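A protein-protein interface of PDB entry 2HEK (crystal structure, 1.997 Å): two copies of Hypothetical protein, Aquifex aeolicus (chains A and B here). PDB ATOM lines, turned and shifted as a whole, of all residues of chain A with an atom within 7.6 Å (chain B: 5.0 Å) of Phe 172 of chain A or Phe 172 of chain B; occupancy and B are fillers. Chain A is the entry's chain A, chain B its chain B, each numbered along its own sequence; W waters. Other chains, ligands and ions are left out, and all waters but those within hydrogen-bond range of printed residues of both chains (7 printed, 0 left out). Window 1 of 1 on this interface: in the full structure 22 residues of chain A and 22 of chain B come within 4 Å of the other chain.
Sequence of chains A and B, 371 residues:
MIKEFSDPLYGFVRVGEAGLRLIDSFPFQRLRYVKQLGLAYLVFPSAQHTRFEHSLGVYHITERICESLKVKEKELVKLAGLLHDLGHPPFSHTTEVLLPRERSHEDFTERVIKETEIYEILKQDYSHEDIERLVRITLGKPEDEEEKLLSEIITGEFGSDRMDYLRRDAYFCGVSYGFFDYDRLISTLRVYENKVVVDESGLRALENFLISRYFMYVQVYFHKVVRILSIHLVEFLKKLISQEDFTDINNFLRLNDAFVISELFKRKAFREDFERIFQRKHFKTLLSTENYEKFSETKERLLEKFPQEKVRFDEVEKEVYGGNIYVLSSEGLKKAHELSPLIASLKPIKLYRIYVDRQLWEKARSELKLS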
ATOM      1  N   SER A   6      -2.254   8.124   5.118  1.00  0.00           N
ATOM      2  CA  SER A   6      -3.243   8.917   5.869  1.00  0.00           C
ATOM      3  C   SER A   6      -3.750  10.013   4.986  1.00  0.00           C
ATOM      4  O   SER A   6      -2.950  10.695   4.327  1.00  0.00           O
ATOM      5  CB  SER A   6      -2.646   9.616   7.118  1.00  0.00           C
ATOM      6  OG  SER A   6      -2.272   8.665   8.080  1.00  0.00           O
ATOM      7  N   ASP A   7      -5.064  10.214   5.013  1.00  0.00           N
ATOM      8  CA  ASP A   7      -5.687  11.316   4.265  1.00  0.00           C
ATOM      9  C   ASP A   7      -6.837  11.757   5.126  1.00  0.00           C
ATOM     10  O   ASP A   7      -7.790  10.989   5.302  1.00  0.00           O
ATOM     11  CB  ASP A   7      -6.197  10.835   2.884  1.00  0.00           C
ATOM     12  CG  ASP A   7      -6.716  11.994   1.995  1.00  0.00           C
ATOM     13  OD1 ASP A   7      -7.102  13.061   2.532  1.00  0.00           O
ATOM     14  OD2 ASP A   7      -6.760  11.833   0.732  1.00  0.00           O
ATOM     15  N   PRO A   8      -6.779  12.997   5.662  1.00  0.00           N
ATOM     16  CA  PRO A   8      -7.851  13.451   6.577  1.00  0.00           C
ATOM     17  C   PRO A   8      -9.228  13.492   5.910  1.00  0.00           C
ATOM     18  O   PRO A   8     -10.242  13.481   6.619  1.00  0.00           O
ATOM     19  CB  PRO A   8      -7.411  14.874   6.962  1.00  0.00           C
ATOM     20  CG  PRO A   8      -6.462  15.307   5.858  1.00  0.00           C
ATOM     21  CD  PRO A   8      -5.747  14.033   5.467  1.00  0.00           C
ATOM     22  N   LEU A   9      -9.292  13.487   4.563  1.00  0.00           N
ATOM     23  CA  LEU A   9     -10.591  13.449   3.906  1.00  0.00           C
ATOM     24  C   LEU A   9     -11.223  12.057   3.986  1.00  0.00           C
ATOM     25  O   LEU A   9     -12.433  11.933   4.000  1.00  0.00           O
ATOM     26  CB  LEU A   9     -10.485  13.869   2.428  1.00  0.00           C
ATOM     27  CG  LEU A   9     -10.643  15.368   2.159  1.00  0.00           C
ATOM     28  CD1 LEU A   9      -9.552  16.247   2.845  1.00  0.00           C
ATOM     29  CD2 LEU A   9     -10.614  15.467   0.685  1.00  0.00           C
ATOM     30  N   LEU A  37      -4.285  25.141  -5.012  1.00  0.00           N
ATOM     31  CA  LEU A  37      -4.974  26.404  -5.254  1.00  0.00           C
ATOM     32  C   LEU A  37      -4.052  27.609  -5.482  1.00  0.00           C
ATOM     33  O   LEU A  37      -4.499  28.738  -5.383  1.00  0.00           O
ATOM     34  CB  LEU A  37      -5.971  26.700  -4.113  1.00  0.00           C
ATOM     35  CG  LEU A  37      -7.143  25.740  -3.900  1.00  0.00           C
ATOM     36  CD1 LEU A  37      -8.051  26.217  -2.734  1.00  0.00           C
ATOM     37  CD2 LEU A  37      -8.007  25.628  -5.151  1.00  0.00           C
ATOM     38  N   PHE A  44      -6.828  32.543   2.141  1.00  0.00           N
ATOM     39  CA  PHE A  44      -7.321  31.420   3.001  1.00  0.00           C
ATOM     40  C   PHE A  44      -6.078  30.709   3.518  1.00  0.00           C
ATOM     41  O   PHE A  44      -5.524  29.873   2.811  1.00  0.00           O
ATOM     42  CB  PHE A  44      -8.178  30.415   2.186  1.00  0.00           C
ATOM     43  CG  PHE A  44      -9.478  30.999   1.713  1.00  0.00           C
ATOM     44  CD1 PHE A  44      -9.560  31.687   0.482  1.00  0.00           C
ATOM     45  CD2 PHE A  44     -10.629  30.907   2.521  1.00  0.00           C
ATOM     46  CE1 PHE A  44     -10.782  32.293   0.074  1.00  0.00           C
ATOM     47  CE2 PHE A  44     -11.859  31.510   2.099  1.00  0.00           C
ATOM     48  CZ  PHE A  44     -11.924  32.170   0.884  1.00  0.00           C
ATOM     49  N   PRO A  45      -5.573  31.106   4.703  1.00  0.00           N
ATOM     50  CA  PRO A  45      -4.197  30.727   5.075  1.00  0.00           C
ATOM     51  C   PRO A  45      -3.914  29.223   5.113  1.00  0.00           C
ATOM     52  O   PRO A  45      -2.787  28.808   4.822  1.00  0.00           O
ATOM     53  CB  PRO A  45      -4.033  31.365   6.480  1.00  0.00           C
ATOM     54  CG  PRO A  45      -4.918  32.583   6.398  1.00  0.00           C
ATOM     55  CD  PRO A  45      -6.150  32.035   5.696  1.00  0.00           C
ATOM     56  N   SER A  46      -4.937  28.425   5.396  1.00  0.00           N
ATOM     57  CA  SER A  46      -4.752  26.966   5.555  1.00  0.00           C
ATOM     58  C   SER A  46      -4.843  26.205   4.204  1.00  0.00           C
ATOM     59  O   SER A  46      -4.732  24.978   4.190  1.00  0.00           O
ATOM     60  CB  SER A  46      -5.775  26.445   6.553  1.00  0.00           C
ATOM     61  OG  SER A  46      -5.455  26.891   7.894  1.00  0.00           O
ATOM     62  N   ALA A  47      -4.995  26.931   3.082  1.00  0.00           N
ATOM     63  CA  ALA A  47      -5.066  26.307   1.727  1.00  0.00           C
ATOM     64  C   ALA A  47      -3.695  25.857   1.272  1.00  0.00           C
ATOM     65  O   ALA A  47      -3.222  26.272   0.202  1.00  0.00           O
ATOM     66  CB  ALA A  47      -5.660  27.288   0.662  1.00  0.00           C
ATOM     67  N   GLN A  48      -3.086  24.959   2.035  1.00  0.00           N
ATOM     68  CA  GLN A  48      -1.695  24.535   1.763  1.00  0.00           C
ATOM     69  C   GLN A  48      -1.628  23.183   1.051  1.00  0.00           C
ATOM     70  O   GLN A  48      -0.549  22.709   0.753  1.00  0.00           O
ATOM     71  CB  GLN A  48      -0.940  24.417   3.105  1.00  0.00           C
ATOM     72  CG  GLN A  48      -0.876  25.727   3.905  1.00  0.00           C
ATOM     73  CD  GLN A  48       0.070  26.697   3.272  1.00  0.00           C
ATOM     74  OE1 GLN A  48      -0.049  27.881   3.444  1.00  0.00           O
ATOM     75  NE2 GLN A  48       1.008  26.190   2.517  1.00  0.00           N
ATOM     76  N   HIS A  49      -2.778  22.554   0.804  1.00  0.00           N
ATOM     77  CA  HIS A  49      -2.796  21.209   0.202  1.00  0.00           C
ATOM     78  C   HIS A  49      -2.214  21.250  -1.224  1.00  0.00           C
ATOM     79  O   HIS A  49      -2.301  22.304  -1.934  1.00  0.00           O
ATOM     80  CB  HIS A  49      -4.218  20.645   0.167  1.00  0.00           C
ATOM     81  CG  HIS A  49      -5.244  21.627  -0.338  1.00  0.00           C
ATOM     82  ND1 HIS A  49      -6.129  21.338  -1.365  1.00  0.00           N
ATOM     83  CD2 HIS A  49      -5.529  22.889   0.056  1.00  0.00           C
ATOM     84  CE1 HIS A  49      -6.915  22.379  -1.574  1.00  0.00           C
ATOM     85  NE2 HIS A  49      -6.552  23.345  -0.744  1.00  0.00           N
ATOM     86  N   THR A  50      -1.597  20.133  -1.636  1.00  0.00           N
ATOM     87  CA  THR A  50      -0.914  20.090  -2.934  1.00  0.00           C
ATOM     88  C   THR A  50      -1.552  19.127  -3.913  1.00  0.00           C
ATOM     89  O   THR A  50      -2.448  18.340  -3.536  1.00  0.00           O
ATOM     90  CB  THR A  50       0.578  19.726  -2.783  1.00  0.00           C
ATOM     91  OG1 THR A  50       0.688  18.319  -2.592  1.00  0.00           O
ATOM     92  CG2 THR A  50       1.204  20.412  -1.581  1.00  0.00           C
ATOM     93  N   GLU A  53      -1.453  15.215  -2.901  1.00  0.00           N
ATOM     94  CA  GLU A  53      -2.530  14.603  -2.121  1.00  0.00           C
ATOM     95  C   GLU A  53      -3.824  14.529  -2.889  1.00  0.00           C
ATOM     96  O   GLU A  53      -4.587  13.560  -2.732  1.00  0.00           O
ATOM     97  CB  GLU A  53      -2.778  15.350  -0.803  1.00  0.00           C
ATOM     98  CG  GLU A  53      -1.526  15.532   0.080  1.00  0.00           C
ATOM     99  CD  GLU A  53      -0.803  16.851  -0.184  1.00  0.00           C
ATOM    100  OE1 GLU A  53      -1.348  17.940   0.169  1.00  0.00           O
ATOM    101  OE2 GLU A  53       0.318  16.780  -0.731  1.00  0.00           O
ATOM    102  N   LEU A 166     -13.353  19.465  -4.672  1.00  0.00           N
ATOM    103  CA  LEU A 166     -14.359  20.283  -3.984  1.00  0.00           C
ATOM    104  C   LEU A 166     -14.288  20.027  -2.493  1.00  0.00           C
ATOM    105  O   LEU A 166     -14.255  20.965  -1.698  1.00  0.00           O
ATOM    106  CB  LEU A 166     -15.789  20.024  -4.488  1.00  0.00           C
ATOM    107  CG  LEU A 166     -16.097  20.545  -5.903  1.00  0.00           C
ATOM    108  CD1 LEU A 166     -17.491  19.995  -6.310  1.00  0.00           C
ATOM    109  CD2 LEU A 166     -16.039  22.113  -5.949  1.00  0.00           C
ATOM    110  N   ARG A 167     -14.262  18.749  -2.117  1.00  0.00           N
ATOM    111  CA  ARG A 167     -14.143  18.343  -0.688  1.00  0.00           C
ATOM    112  C   ARG A 167     -12.810  18.752  -0.054  1.00  0.00           C
ATOM    113  O   ARG A 167     -12.758  19.237   1.093  1.00  0.00           O
ATOM    114  CB  ARG A 167     -14.411  16.824  -0.529  1.00  0.00           C
ATOM    115  CG  ARG A 167     -14.279  16.228   0.929  1.00  0.00           C
ATOM    116  CD  ARG A 167     -14.731  14.633   1.129  1.00  0.00           C
ATOM    117  NE  ARG A 167     -14.825  14.388   2.558  1.00  0.00           N
ATOM    118  CZ  ARG A 167     -15.404  13.326   3.065  1.00  0.00           C
ATOM    119  NH1 ARG A 167     -15.951  12.421   2.250  1.00  0.00           N
ATOM    120  NH2 ARG A 167     -15.464  13.179   4.372  1.00  0.00           N
ATOM    121  N   ARG A 168     -11.701  18.537  -0.751  1.00  0.00           N
ATOM    122  CA  ARG A 168     -10.406  18.867  -0.184  1.00  0.00           C
ATOM    123  C   ARG A 168     -10.232  20.407  -0.044  1.00  0.00           C
ATOM    124  O   ARG A 168      -9.711  20.903   0.977  1.00  0.00           O
ATOM    125  CB  ARG A 168      -9.281  18.245  -1.061  1.00  0.00           C
ATOM    126  CG  ARG A 168      -7.832  18.357  -0.477  1.00  0.00           C
ATOM    127  CD  ARG A 168      -6.769  17.537  -1.325  1.00  0.00           C
ATOM    128  NE  ARG A 168      -7.292  16.176  -1.500  1.00  0.00           N
ATOM    129  CZ  ARG A 168      -7.146  15.194  -0.620  1.00  0.00           C
ATOM    130  NH1 ARG A 168      -6.408  15.364   0.482  1.00  0.00           N
ATOM    131  NH2 ARG A 168      -7.744  14.045  -0.847  1.00  0.00           N
ATOM    132  N   ASP A 169     -10.651  21.157  -1.076  1.00  0.00           N
ATOM    133  CA  ASP A 169     -10.588  22.619  -1.047  1.00  0.00           C
ATOM    134  C   ASP A 169     -11.407  23.132   0.134  1.00  0.00           C
ATOM    135  O   ASP A 169     -10.935  23.995   0.856  1.00  0.00           O
ATOM    136  CB  ASP A 169     -11.069  23.239  -2.371  1.00  0.00           C
ATOM    137  CG  ASP A 169     -10.138  22.915  -3.562  1.00  0.00           C
ATOM    138  OD1 ASP A 169      -9.042  22.363  -3.361  1.00  0.00           O
ATOM    139  OD2 ASP A 169     -10.515  23.204  -4.714  1.00  0.00           O
ATOM    140  N   ALA A 170     -12.590  22.553   0.370  1.00  0.00           N
ATOM    141  CA  ALA A 170     -13.465  22.997   1.479  1.00  0.00           C
ATOM    142  C   ALA A 170     -12.785  22.679   2.802  1.00  0.00           C
ATOM    143  O   ALA A 170     -12.799  23.477   3.706  1.00  0.00           O
ATOM    144  CB  ALA A 170     -14.794  22.298   1.427  1.00  0.00           C
ATOM    145  N   TYR A 171     -12.200  21.489   2.908  1.00  0.00           N
ATOM    146  CA  TYR A 171     -11.594  21.007   4.148  1.00  0.00           C
ATOM    147  C   TYR A 171     -10.424  21.901   4.547  1.00  0.00           C
ATOM    148  O   TYR A 171     -10.276  22.257   5.711  1.00  0.00           O
ATOM    149  CB  TYR A 171     -11.093  19.555   3.945  1.00  0.00           C
ATOM    150  CG  TYR A 171     -10.560  18.900   5.199  1.00  0.00           C
ATOM    151  CD1 TYR A 171     -11.433  18.237   6.078  1.00  0.00           C
ATOM    152  CD2 TYR A 171      -9.165  18.909   5.491  1.00  0.00           C
ATOM    153  CE1 TYR A 171     -10.952  17.625   7.261  1.00  0.00           C
ATOM    154  CE2 TYR A 171      -8.660  18.250   6.628  1.00  0.00           C
ATOM    155  CZ  TYR A 171      -9.591  17.616   7.512  1.00  0.00           C
ATOM    156  OH  TYR A 171      -9.162  17.010   8.677  1.00  0.00           O
ATOM    157  N   PHE A 172      -9.579  22.264   3.592  1.00  0.00           N
ATOM    158  CA  PHE A 172      -8.383  23.056   3.921  1.00  0.00           C
ATOM    159  C   PHE A 172      -8.665  24.553   3.947  1.00  0.00           C
ATOM    160  O   PHE A 172      -8.068  25.265   4.740  1.00  0.00           O
ATOM    161  CB  PHE A 172      -7.230  22.793   2.933  1.00  0.00           C
ATOM    162  CG  PHE A 172      -6.543  21.466   3.147  1.00  0.00           C
ATOM    163  CD1 PHE A 172      -7.101  20.285   2.668  1.00  0.00           C
ATOM    164  CD2 PHE A 172      -5.322  21.400   3.800  1.00  0.00           C
ATOM    165  CE1 PHE A 172      -6.484  19.052   2.867  1.00  0.00           C
ATOM    166  CE2 PHE A 172      -4.680  20.128   3.998  1.00  0.00           C
ATOM    167  CZ  PHE A 172      -5.302  18.965   3.543  1.00  0.00           C
ATOM    168  N   CYS A 173      -9.504  25.061   3.050  1.00  0.00           N
ATOM    169  CA  CYS A 173      -9.835  26.514   3.122  1.00  0.00           C
ATOM    170  C   CYS A 173     -10.628  26.854   4.359  1.00  0.00           C
ATOM    171  O   CYS A 173     -10.461  27.949   4.894  1.00  0.00           O
ATOM    172  CB  CYS A 173     -10.584  27.031   1.891  1.00  0.00           C
ATOM    173  SG  CYS A 173      -9.566  26.972   0.411  1.00  0.00           S
ATOM    174  N   GLY A 174     -11.457  25.908   4.810  1.00  0.00           N
ATOM    175  CA  GLY A 174     -12.359  26.099   5.969  1.00  0.00           C
ATOM    176  C   GLY A 174     -13.739  26.587   5.524  1.00  0.00           C
ATOM    177  O   GLY A 174     -14.278  27.491   6.123  1.00  0.00           O
ATOM    178  N   VAL A 175     -14.332  25.971   4.495  1.00  0.00           N
ATOM    179  CA  VAL A 175     -15.616  26.406   3.979  1.00  0.00           C
ATOM    180  C   VAL A 175     -16.705  25.495   4.534  1.00  0.00           C
ATOM    181  O   VAL A 175     -16.936  24.415   4.046  1.00  0.00           O
ATOM    182  CB  VAL A 175     -15.614  26.509   2.423  1.00  0.00           C
ATOM    183  CG1 VAL A 175     -16.986  26.992   1.889  1.00  0.00           C
ATOM    184  CG2 VAL A 175     -14.540  27.482   1.992  1.00  0.00           C
ATOM    185  N   MET A 216     -18.342  26.704  -3.150  1.00  0.00           N
ATOM    186  CA  MET A 216     -16.901  26.804  -3.386  1.00  0.00           C
ATOM    187  C   MET A 216     -16.567  27.921  -4.374  1.00  0.00           C
ATOM    188  O   MET A 216     -15.573  28.626  -4.188  1.00  0.00           O
ATOM    189  CB  MET A 216     -16.305  25.472  -3.840  1.00  0.00           C
ATOM    190  CG  MET A 216     -16.333  24.393  -2.734  1.00  0.00           C
ATOM    191  SD  MET A 216     -15.508  24.964  -1.180  1.00  0.00           S
ATOM    192  CE  MET A 216     -13.856  25.294  -1.738  1.00  0.00           C
ATOM    193  N   PRO B   8     -10.022  26.473   9.284  1.00  0.00           N
ATOM    194  CA  PRO B   8     -10.883  25.282   9.380  1.00  0.00           C
ATOM    195  C   PRO B   8     -10.904  24.686  10.778  1.00  0.00           C
ATOM    196  O   PRO B   8     -11.806  23.873  11.100  1.00  0.00           O
ATOM    197  CB  PRO B   8     -10.233  24.293   8.411  1.00  0.00           C
ATOM    198  CG  PRO B   8      -8.804  24.752   8.245  1.00  0.00           C
ATOM    199  CD  PRO B   8      -8.930  26.279   8.321  1.00  0.00           C
ATOM    200  N   LEU B   9      -9.943  25.088  11.615  1.00  0.00           N
ATOM    201  CA  LEU B   9      -9.912  24.598  13.015  1.00  0.00           C
ATOM    202  C   LEU B   9     -10.921  25.317  13.900  1.00  0.00           C
ATOM    203  O   LEU B   9     -11.308  24.775  14.921  1.00  0.00           O
ATOM    204  CB  LEU B   9      -8.501  24.666  13.653  1.00  0.00           C
ATOM    205  CG  LEU B   9      -7.465  23.543  13.433  1.00  0.00           C
ATOM    206  CD1 LEU B   9      -8.051  22.246  13.967  1.00  0.00           C
ATOM    207  CD2 LEU B   9      -7.150  23.309  11.912  1.00  0.00           C
ATOM    208  N   SER B  46      -0.766  15.024   3.895  1.00  0.00           N
ATOM    209  CA  SER B  46      -1.546  16.270   4.078  1.00  0.00           C
ATOM    210  C   SER B  46      -0.978  17.194   5.171  1.00  0.00           C
ATOM    211  O   SER B  46      -1.543  18.255   5.432  1.00  0.00           O
ATOM    212  CB  SER B  46      -2.996  15.936   4.360  1.00  0.00           C
ATOM    213  OG  SER B  46      -3.593  15.382   3.191  1.00  0.00           O
ATOM    214  N   ALA B  47       0.165  16.841   5.755  1.00  0.00           N
ATOM    215  CA  ALA B  47       0.749  17.691   6.844  1.00  0.00           C
ATOM    216  C   ALA B  47       1.495  18.901   6.266  1.00  0.00           C
ATOM    217  O   ALA B  47       2.708  19.029   6.415  1.00  0.00           O
ATOM    218  CB  ALA B  47       1.661  16.863   7.793  1.00  0.00           C
ATOM    219  N   GLN B  48       0.742  19.775   5.599  1.00  0.00           N
ATOM    220  CA  GLN B  48       1.270  20.921   4.836  1.00  0.00           C
ATOM    221  C   GLN B  48       1.093  22.255   5.556  1.00  0.00           C
ATOM    222  O   GLN B  48       1.551  23.314   5.053  1.00  0.00           O
ATOM    223  CB  GLN B  48       0.546  21.016   3.466  1.00  0.00           C
ATOM    224  CG  GLN B  48       0.683  19.755   2.586  1.00  0.00           C
ATOM    225  CD  GLN B  48       2.058  19.605   1.952  1.00  0.00           C
ATOM    226  OE1 GLN B  48       2.499  18.483   1.645  1.00  0.00           O
ATOM    227  NE2 GLN B  48       2.741  20.723   1.745  1.00  0.00           N
ATOM    228  N   HIS B  49       0.423  22.210   6.704  1.00  0.00           N
ATOM    229  CA  HIS B  49       0.171  23.430   7.487  1.00  0.00           C
ATOM    230  C   HIS B  49       1.481  24.090   7.973  1.00  0.00           C
ATOM    231  O   HIS B  49       2.483  23.400   8.219  1.00  0.00           O
ATOM    232  CB  HIS B  49      -0.765  23.133   8.660  1.00  0.00           C
ATOM    233  CG  HIS B  49      -0.277  22.038   9.574  1.00  0.00           C
ATOM    234  ND1 HIS B  49      -0.072  20.741   9.147  1.00  0.00           N
ATOM    235  CD2 HIS B  49      -0.014  22.043  10.909  1.00  0.00           C
ATOM    236  CE1 HIS B  49       0.305  19.995  10.179  1.00  0.00           C
ATOM    237  NE2 HIS B  49       0.351  20.765  11.261  1.00  0.00           N
ATOM    238  N   ARG B 168      -4.528  21.231  15.369  1.00  0.00           N
ATOM    239  CA  ARG B 168      -4.134  21.500  13.984  1.00  0.00           C
ATOM    240  C   ARG B 168      -3.348  20.322  13.389  1.00  0.00           C
ATOM    241  O   ARG B 168      -3.580  19.919  12.226  1.00  0.00           O
ATOM    242  CB  ARG B 168      -3.307  22.814  13.875  1.00  0.00           C
ATOM    243  CG  ARG B 168      -3.082  23.330  12.431  1.00  0.00           C
ATOM    244  CD  ARG B 168      -2.427  24.787  12.382  1.00  0.00           C
ATOM    245  NE  ARG B 168      -3.278  25.655  13.226  1.00  0.00           N
ATOM    246  CZ  ARG B 168      -4.406  26.230  12.812  1.00  0.00           C
ATOM    247  NH1 ARG B 168      -4.811  26.119  11.537  1.00  0.00           N
ATOM    248  NH2 ARG B 168      -5.131  26.913  13.658  1.00  0.00           N
ATOM    249  N   ASP B 169      -2.398  19.783  14.151  1.00  0.00           N
ATOM    250  CA  ASP B 169      -1.632  18.610  13.665  1.00  0.00           C
ATOM    251  C   ASP B 169      -2.576  17.430  13.412  1.00  0.00           C
ATOM    252  O   ASP B 169      -2.459  16.751  12.381  1.00  0.00           O
ATOM    253  CB  ASP B 169      -0.497  18.207  14.620  1.00  0.00           C
ATOM    254  CG  ASP B 169       0.542  19.288  14.774  1.00  0.00           C
ATOM    255  OD1 ASP B 169       0.551  20.266  13.998  1.00  0.00           O
ATOM    256  OD2 ASP B 169       1.326  19.170  15.722  1.00  0.00           O
ATOM    257  N   ALA B 170      -3.549  17.219  14.298  1.00  0.00           N
ATOM    258  CA  ALA B 170      -4.505  16.122  14.089  1.00  0.00           C
ATOM    259  C   ALA B 170      -5.319  16.317  12.813  1.00  0.00           C
ATOM    260  O   ALA B 170      -5.594  15.342  12.077  1.00  0.00           O
ATOM    261  CB  ALA B 170      -5.449  16.004  15.262  1.00  0.00           C
ATOM    262  N   TYR B 171      -5.745  17.566  12.576  1.00  0.00           N
ATOM    263  CA  TYR B 171      -6.641  17.915  11.462  1.00  0.00           C
ATOM    264  C   TYR B 171      -5.972  17.694  10.096  1.00  0.00           C
ATOM    265  O   TYR B 171      -6.611  17.218   9.143  1.00  0.00           O
ATOM    266  CB  TYR B 171      -7.013  19.424  11.571  1.00  0.00           C
ATOM    267  CG  TYR B 171      -8.139  19.870  10.630  1.00  0.00           C
ATOM    268  CD1 TYR B 171      -9.485  19.650  10.961  1.00  0.00           C
ATOM    269  CD2 TYR B 171      -7.838  20.516   9.405  1.00  0.00           C
ATOM    270  CE1 TYR B 171     -10.540  20.056  10.073  1.00  0.00           C
ATOM    271  CE2 TYR B 171      -8.849  20.922   8.522  1.00  0.00           C
ATOM    272  CZ  TYR B 171     -10.196  20.699   8.871  1.00  0.00           C
ATOM    273  OH  TYR B 171     -11.176  21.098   7.976  1.00  0.00           O
ATOM    274  N   PHE B 172      -4.712  18.117   9.999  1.00  0.00           N
ATOM    275  CA  PHE B 172      -3.941  17.989   8.757  1.00  0.00           C
ATOM    276  C   PHE B 172      -3.304  16.612   8.545  1.00  0.00           C
ATOM    277  O   PHE B 172      -3.265  16.123   7.438  1.00  0.00           O
ATOM    278  CB  PHE B 172      -2.875  19.078   8.654  1.00  0.00           C
ATOM    279  CG  PHE B 172      -3.439  20.430   8.309  1.00  0.00           C
ATOM    280  CD1 PHE B 172      -3.375  20.912   6.993  1.00  0.00           C
ATOM    281  CD2 PHE B 172      -4.032  21.220   9.291  1.00  0.00           C
ATOM    282  CE1 PHE B 172      -3.914  22.206   6.665  1.00  0.00           C
ATOM    283  CE2 PHE B 172      -4.562  22.497   9.000  1.00  0.00           C
ATOM    284  CZ  PHE B 172      -4.543  22.985   7.701  1.00  0.00           C
ATOM    285  N   CYS B 173      -2.771  15.992   9.588  1.00  0.00           N
ATOM    286  CA  CYS B 173      -2.155  14.673   9.419  1.00  0.00           C
ATOM    287  C   CYS B 173      -3.242  13.669   9.141  1.00  0.00           C
ATOM    288  O   CYS B 173      -3.021  12.717   8.394  1.00  0.00           O
ATOM    289  CB  CYS B 173      -1.387  14.252  10.695  1.00  0.00           C
ATOM    290  SG  CYS B 173       0.130  15.179  10.854  1.00  0.00           S
ATOM    291  N   GLY B 174      -4.407  13.891   9.741  1.00  0.00           N
ATOM    292  CA  GLY B 174      -5.548  12.950   9.629  1.00  0.00           C
ATOM    293  C   GLY B 174      -5.564  11.983  10.799  1.00  0.00           C
ATOM    294  O   GLY B 174      -5.647  10.772  10.590  1.00  0.00           O
HETATM  295  O   HOH W   1       2.493  15.741   0.428  1.00  0.00           O
HETATM  296  O   HOH W   2       3.167  24.189   3.150  1.00  0.00           O
HETATM  297  O   HOH W   3      -3.051  12.871   2.342  1.00  0.00           O
HETATM  298  O   HOH W   4       2.118  23.323   0.619  1.00  0.00           O
HETATM  299  O   HOH W   5      -3.382  25.480   8.940  1.00  0.00           O
HETATM  300  O   HOH W   6      -1.739  12.952   5.804  1.00  0.00           O
HETATM  301  O   HOH W   7      -4.214  17.286   1.312  1.00  0.00           O
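Pro 8 of chain A touches Phe 172 of chain B.
CB of Pro 8 of chain A touches CA of Gly 174 of chain B, at 3.8 Å.
Gln 48 of chain B touches Gln 48 of chain A (O to CB, 3.3 Å).
OG of Ser 46 of chain B touches CG of Glu 53 of chain A, at 3.7 Å.
Ser 46 of chain B touches Arg 168 of chain A (OG to NH1, 3.9 Å).
Tyr 171 of chain A touches Pro 8 of chain B.
Phe 172 of chain A touches Ser 46 of chain B (CZ to CB, 3.9 Å).
Of the printed residues of chain B, Ser 6 of chain A touches Cys 173 (3.4 Å).
Of the printed residues of chain B, Ser 46 of chain A touches Pro 8 (3.6 Å), Arg 168 (3.8 Å) and Phe 172 (3.8 Å).
Of the printed residues of chain B, Tyr 171 of chain A touches Pro 8 and Tyr 171.
Phe 172 of chain A touches just these residues of chain B: Pro 8, Ser 46 and Phe 172.
Met 216 of chain A touches none of the printed residues of chain B.
Phe 172 of chain B touches just these residues of chain A: Pro 8, Ser 46 and Phe 172.
The nearest residue of chain B that does not touch Phe 172 of chain A is Tyr 171 of chain B (4.8 Å).
Pro 8 of chain A touches Phe 172 of chain B, and with the chains exchanged Phe 172 of chain A touches Pro 8 of chain B.
Ser 46 of chain A touches Arg 168 of chain B, and with the chains exchanged Arg 168 of chain A touches Ser 46 of chain B.
Tyr 171 of chain B touches its own counterpart, Tyr 171 of chain A.
Phe 172 of chain B touches its own counterpart, Phe 172 of chain A.
Printed residues of chain B that touch a printed residue of chain A: Pro 8, Ser 46, Gln 48, Arg 168, Tyr 171, Phe 172, Cys 173 and Gly 174.
Hydrophobic or aromatic side chains of chain B that line the printed part of chain A: Pro 8, Tyr 171 and Phe 172.
Printed residues of chain A that touch a printed residue of chain B: Ser 6, Pro 8, Ser 46, Gln 48, Thr 50, Glu 53, Arg 168, Tyr 171, Phe 172 and Gly 174.
Hydrophobic or aromatic side chains of chain A within 4 Å of the printed part of chain B: Pro 8, Tyr 171 and Phe 172.
Among the printed residues, 19 pairs touch across the chains.
Water W3 bridges OG of Ser 46 of chain B (2.7 Å) and O of Ser 6 of chain A (2.9 Å).
Water W5 lies within hydrogen-bond range of the side-chain hydroxyl of Ser 46 of chain A (2.7 Å) and the guanidinium group of Arg 168 of chain B (3.0 Å).
Water W6 lies within hydrogen-bond range of O of Cys 173 of chain B (2.9 Å), O of Ser 6 of chain A (3.0 Å) and N of Ser 46 of chain B (3.0 Å).
O of Tyr 171 of chain B is in hydrogen-bond range of OH of Tyr 171 of chain A.
The side-chain sulfur of Cys 173 of chain B lies close to the backbone carbonyl oxygen of Asp 169 of chain B, at 3.4 Å.
The side-chain carboxylate (OE2) of Glu 53 of chain A sits at hydrogen-bond distance from the side-chain hydroxyl (OG1) of Thr 50 of chain A (2.4 Å).
The side-chain carboxylate of Asp 7 of chain A is in salt-bridge range of the guanidinium group of Arg 168 of chain A (2.9 Å).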
